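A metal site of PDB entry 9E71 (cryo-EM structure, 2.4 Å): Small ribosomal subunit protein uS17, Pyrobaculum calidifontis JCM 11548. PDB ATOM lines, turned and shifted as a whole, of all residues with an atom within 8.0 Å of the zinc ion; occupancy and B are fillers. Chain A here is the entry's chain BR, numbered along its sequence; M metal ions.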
ATOM      1  N   THR A   2       9.279   9.259 -11.311  1.00  0.00           N
ATOM      2  CA  THR A   2       8.083   9.425 -10.491  1.00  0.00           C
ATOM      3  C   THR A   2       8.357   9.020  -9.048  1.00  0.00           C
ATOM      4  O   THR A   2       7.920   9.703  -8.109  1.00  0.00           O
ATOM      5  CB  THR A   2       6.902   8.602 -11.032  1.00  0.00           C
ATOM      6  OG1 THR A   2       6.328   9.290 -12.147  1.00  0.00           O
ATOM      7  CG2 THR A   2       5.851   8.415  -9.949  1.00  0.00           C
ATOM      8  N   VAL A   3       9.080   7.923  -8.868  1.00  0.00           N
ATOM      9  CA  VAL A   3       9.454   7.417  -7.562  1.00  0.00           C
ATOM     10  C   VAL A   3      10.962   7.158  -7.555  1.00  0.00           C
ATOM     11  O   VAL A   3      11.523   6.653  -8.524  1.00  0.00           O
ATOM     12  CB  VAL A   3       8.695   6.130  -7.196  1.00  0.00           C
ATOM     13  CG1 VAL A   3       8.981   5.040  -8.214  1.00  0.00           C
ATOM     14  CG2 VAL A   3       9.079   5.664  -5.814  1.00  0.00           C
ATOM     15  N   VAL A  24      11.553  17.388  -3.696  1.00  0.00           N
ATOM     16  CA  VAL A  24      10.401  16.986  -2.912  1.00  0.00           C
ATOM     17  C   VAL A  24      10.781  17.125  -1.451  1.00  0.00           C
ATOM     18  O   VAL A  24      11.796  16.556  -1.017  1.00  0.00           O
ATOM     19  CB  VAL A  24       9.961  15.542  -3.211  1.00  0.00           C
ATOM     20  CG1 VAL A  24       8.444  15.420  -3.166  1.00  0.00           C
ATOM     21  CG2 VAL A  24      10.523  15.075  -4.548  1.00  0.00           C
ATOM     22  N   PRO A  37       8.265   7.162   4.422  1.00  0.00           N
ATOM     23  CA  PRO A  37       8.739   5.988   3.690  1.00  0.00           C
ATOM     24  C   PRO A  37      10.175   6.151   3.240  1.00  0.00           C
ATOM     25  O   PRO A  37      10.736   7.247   3.218  1.00  0.00           O
ATOM     26  CB  PRO A  37       7.793   5.913   2.485  1.00  0.00           C
ATOM     27  CG  PRO A  37       7.341   7.312   2.277  1.00  0.00           C
ATOM     28  CD  PRO A  37       7.432   8.041   3.580  1.00  0.00           C
ATOM     29  N   ALA A  39      11.215   5.916   0.306  1.00  0.00           N
ATOM     30  CA  ALA A  39      11.231   6.371  -1.077  1.00  0.00           C
ATOM     31  C   ALA A  39      10.395   7.636  -1.172  1.00  0.00           C
ATOM     32  O   ALA A  39       9.507   7.870  -0.351  1.00  0.00           O
ATOM     33  CB  ALA A  39      10.687   5.303  -2.020  1.00  0.00           C
ATOM     34  N   VAL A  40      10.691   8.442  -2.184  1.00  0.00           N
ATOM     35  CA  VAL A  40      10.012   9.706  -2.403  1.00  0.00           C
ATOM     36  C   VAL A  40       9.391   9.693  -3.791  1.00  0.00           C
ATOM     37  O   VAL A  40      10.058   9.323  -4.775  1.00  0.00           O
ATOM     38  CB  VAL A  40      10.985  10.891  -2.264  1.00  0.00           C
ATOM     39  CG1 VAL A  40      10.283  12.181  -2.611  1.00  0.00           C
ATOM     40  CG2 VAL A  40      11.556  10.951  -0.858  1.00  0.00           C
ATOM     41  N   CYS A  41       8.128  10.089  -3.877  1.00  0.00           N
ATOM     42  CA  CYS A  41       7.416  10.188  -5.137  1.00  0.00           C
ATOM     43  C   CYS A  41       7.100  11.652  -5.431  1.00  0.00           C
ATOM     44  O   CYS A  41       7.227  12.530  -4.573  1.00  0.00           O
ATOM     45  CB  CYS A  41       6.147   9.349  -5.123  1.00  0.00           C
ATOM     46  SG  CYS A  41       4.743  10.162  -4.343  1.00  0.00           S
ATOM     47  N   ASP A  42       6.675  11.914  -6.657  1.00  0.00           N
ATOM     48  CA  ASP A  42       6.280  13.253  -7.086  1.00  0.00           C
ATOM     49  C   ASP A  42       4.763  13.410  -7.167  1.00  0.00           C
ATOM     50  O   ASP A  42       4.264  14.348  -7.787  1.00  0.00           O
ATOM     51  CB  ASP A  42       6.981  13.624  -8.398  1.00  0.00           C
ATOM     52  CG  ASP A  42       6.523  12.816  -9.622  1.00  0.00           C
ATOM     53  OD1 ASP A  42       5.322  12.604  -9.910  1.00  0.00           O
ATOM     54  OD2 ASP A  42       7.430  12.336 -10.334  1.00  0.00           O
ATOM     55  N   ASP A  43       4.030  12.489  -6.582  1.00  0.00           N
ATOM     56  CA  ASP A  43       2.577  12.473  -6.717  1.00  0.00           C
ATOM     57  C   ASP A  43       1.974  13.639  -5.943  1.00  0.00           C
ATOM     58  O   ASP A  43       2.198  13.758  -4.743  1.00  0.00           O
ATOM     59  CB  ASP A  43       2.003  11.151  -6.200  1.00  0.00           C
ATOM     60  CG  ASP A  43       0.627  10.858  -6.747  1.00  0.00           C
ATOM     61  OD1 ASP A  43       0.088  11.682  -7.502  1.00  0.00           O
ATOM     62  OD2 ASP A  43       0.072   9.784  -6.429  1.00  0.00           O
ATOM     63  N   PRO A  44       1.185  14.503  -6.596  1.00  0.00           N
ATOM     64  CA  PRO A  44       0.523  15.592  -5.861  1.00  0.00           C
ATOM     65  C   PRO A  44      -0.646  15.129  -5.003  1.00  0.00           C
ATOM     66  O   PRO A  44      -1.201  15.958  -4.274  1.00  0.00           O
ATOM     67  CB  PRO A  44       0.053  16.535  -6.976  1.00  0.00           C
ATOM     68  CG  PRO A  44       0.085  15.742  -8.230  1.00  0.00           C
ATOM     69  CD  PRO A  44       0.912  14.526  -8.039  1.00  0.00           C
ATOM     70  N   LEU A  45      -1.034  13.858  -5.078  1.00  0.00           N
ATOM     71  CA  LEU A  45      -2.040  13.294  -4.188  1.00  0.00           C
ATOM     72  C   LEU A  45      -1.422  12.484  -3.059  1.00  0.00           C
ATOM     73  O   LEU A  45      -2.149  11.835  -2.318  1.00  0.00           O
ATOM     74  CB  LEU A  45      -3.016  12.418  -4.983  1.00  0.00           C
ATOM     75  CG  LEU A  45      -4.054  13.149  -5.818  1.00  0.00           C
ATOM     76  CD1 LEU A  45      -4.664  12.201  -6.844  1.00  0.00           C
ATOM     77  CD2 LEU A  45      -5.131  13.766  -4.942  1.00  0.00           C
ATOM     78  N   CYS A  46      -0.099  12.488  -2.932  1.00  0.00           N
ATOM     79  CA  CYS A  46       0.565  11.814  -1.837  1.00  0.00           C
ATOM     80  C   CYS A  46       0.442  12.642  -0.565  1.00  0.00           C
ATOM     81  O   CYS A  46       0.419  13.868  -0.606  1.00  0.00           O
ATOM     82  CB  CYS A  46       2.043  11.600  -2.177  1.00  0.00           C
ATOM     83  SG  CYS A  46       2.977  10.599  -1.001  1.00  0.00           S
ATOM     84  N   PRO A  47       0.336  11.993   0.593  1.00  0.00           N
ATOM     85  CA  PRO A  47       0.304  12.755   1.844  1.00  0.00           C
ATOM     86  C   PRO A  47       1.698  13.082   2.365  1.00  0.00           C
ATOM     87  O   PRO A  47       1.861  14.024   3.130  1.00  0.00           O
ATOM     88  CB  PRO A  47      -0.450  11.835   2.803  1.00  0.00           C
ATOM     89  CG  PRO A  47      -0.388  10.472   2.209  1.00  0.00           C
ATOM     90  CD  PRO A  47       0.098  10.558   0.795  1.00  0.00           C
ATOM     91  N   TRP A  48       2.710  12.314   1.945  1.00  0.00           N
ATOM     92  CA  TRP A  48       4.082  12.596   2.339  1.00  0.00           C
ATOM     93  C   TRP A  48       4.775  13.565   1.389  1.00  0.00           C
ATOM     94  O   TRP A  48       5.574  14.391   1.839  1.00  0.00           O
ATOM     95  CB  TRP A  48       4.898  11.305   2.401  1.00  0.00           C
ATOM     96  CG  TRP A  48       4.416  10.336   3.396  1.00  0.00           C
ATOM     97  CD1 TRP A  48       3.649   9.248   3.173  1.00  0.00           C
ATOM     98  CD2 TRP A  48       4.677  10.369   4.796  1.00  0.00           C
ATOM     99  NE1 TRP A  48       3.413   8.592   4.354  1.00  0.00           N
ATOM    100  CE2 TRP A  48       4.029   9.260   5.364  1.00  0.00           C
ATOM    101  CE3 TRP A  48       5.394  11.233   5.637  1.00  0.00           C
ATOM    102  CZ2 TRP A  48       4.077   8.991   6.730  1.00  0.00           C
ATOM    103  CZ3 TRP A  48       5.442  10.957   6.982  1.00  0.00           C
ATOM    104  CH2 TRP A  48       4.793   9.852   7.520  1.00  0.00           C
ATOM    105  N   HIS A  49       4.498  13.457   0.090  1.00  0.00           N
ATOM    106  CA  HIS A  49       5.185  14.251  -0.913  1.00  0.00           C
ATOM    107  C   HIS A  49       4.204  15.000  -1.798  1.00  0.00           C
ATOM    108  O   HIS A  49       4.520  15.320  -2.945  1.00  0.00           O
ATOM    109  CB  HIS A  49       6.099  13.364  -1.760  1.00  0.00           C
ATOM    110  CG  HIS A  49       6.756  12.268  -0.983  1.00  0.00           C
ATOM    111  ND1 HIS A  49       6.437  10.941  -1.148  1.00  0.00           N
ATOM    112  CD2 HIS A  49       7.727  12.307  -0.035  1.00  0.00           C
ATOM    113  CE1 HIS A  49       7.165  10.205  -0.336  1.00  0.00           C
ATOM    114  NE2 HIS A  49       7.960  11.010   0.354  1.00  0.00           N
ATOM    115  N   GLY A  50       3.018  15.299  -1.284  1.00  0.00           N
ATOM    116  CA  GLY A  50       2.021  15.985  -2.075  1.00  0.00           C
ATOM    117  C   GLY A  50       1.184  16.948  -1.261  1.00  0.00           C
ATOM    118  O   GLY A  50       1.532  17.271  -0.128  1.00  0.00           O
ATOM    119  N   PRO A 100       0.127   5.006  -2.083  1.00  0.00           N
ATOM    120  CA  PRO A 100       1.048   5.862  -2.832  1.00  0.00           C
ATOM    121  C   PRO A 100       2.206   5.069  -3.421  1.00  0.00           C
ATOM    122  O   PRO A 100       2.464   3.919  -3.074  1.00  0.00           O
ATOM    123  CB  PRO A 100       1.536   6.866  -1.785  1.00  0.00           C
ATOM    124  CG  PRO A 100       0.615   6.753  -0.636  1.00  0.00           C
ATOM    125  CD  PRO A 100      -0.083   5.444  -0.698  1.00  0.00           C
ATOM    126  N   GLU A 101       2.918   5.720  -4.333  1.00  0.00           N
ATOM    127  CA  GLU A 101       3.980   5.045  -5.075  1.00  0.00           C
ATOM    128  C   GLU A 101       5.169   4.723  -4.180  1.00  0.00           C
ATOM    129  O   GLU A 101       5.794   3.668  -4.335  1.00  0.00           O
ATOM    130  CB  GLU A 101       4.440   5.908  -6.255  1.00  0.00           C
ATOM    131  CG  GLU A 101       3.366   6.261  -7.291  1.00  0.00           C
ATOM    132  CD  GLU A 101       2.504   7.440  -6.891  1.00  0.00           C
ATOM    133  OE1 GLU A 101       2.745   7.997  -5.795  1.00  0.00           O
ATOM    134  OE2 GLU A 101       1.606   7.822  -7.655  1.00  0.00           O
ATOM    135  N   CYS A 102       5.498   5.606  -3.246  1.00  0.00           N
ATOM    136  CA  CYS A 102       6.663   5.400  -2.395  1.00  0.00           C
ATOM    137  C   CYS A 102       6.466   4.275  -1.398  1.00  0.00           C
ATOM    138  O   CYS A 102       7.452   3.773  -0.854  1.00  0.00           O
ATOM    139  CB  CYS A 102       6.996   6.704  -1.668  1.00  0.00           C
ATOM    140  SG  CYS A 102       5.582   7.800  -1.427  1.00  0.00           S
ATOM    141  N   ILE A 103       5.231   3.878  -1.125  1.00  0.00           N
ATOM    142  CA  ILE A 103       4.921   2.825  -0.155  1.00  0.00           C
ATOM    143  C   ILE A 103       4.525   1.586  -0.932  1.00  0.00           C
ATOM    144  O   ILE A 103       3.387   1.472  -1.412  1.00  0.00           O
ATOM    145  CB  ILE A 103       3.811   3.247   0.808  1.00  0.00           C
ATOM    146  CG1 ILE A 103       4.131   4.604   1.441  1.00  0.00           C
ATOM    147  CG2 ILE A 103       3.603   2.202   1.887  1.00  0.00           C
ATOM    148  CD1 ILE A 103       3.101   5.053   2.445  1.00  0.00           C
HETATM  149 ZN    ZN M   1       4.912   9.916  -2.060  1.00  0.00          ZN
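The side-chain sulfur (SG) of Cys 41 lies close to the backbone NH (N) of Asp 43, at 3.3 Å.
The side-chain sulfur of Cys 41 lies close to the side-chain carboxylate of Glu 101, 3.3 Å away.
The side-chain sulfur (SG) of Cys 46 lies close to the backbone NH (N) of Trp 48 (3.4 Å).
Of the 20 residues printed, 4 come within 4 Å of the zinc ion.
Along chain A the residues within 4 Å of the zinc ion span positions 41 to 102.
The nearest printed residue that does not touch the zinc ion is Pro 100 (4.6 Å).
The zinc ion is bound by ND1 of His 49 (2.1 Å), SG of Cys 41 (2.3 Å), SG of Cys 102 (2.3 Å) and SG of Cys 46 (2.3 Å).
The zinc ion has four donor atoms within binding distance.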
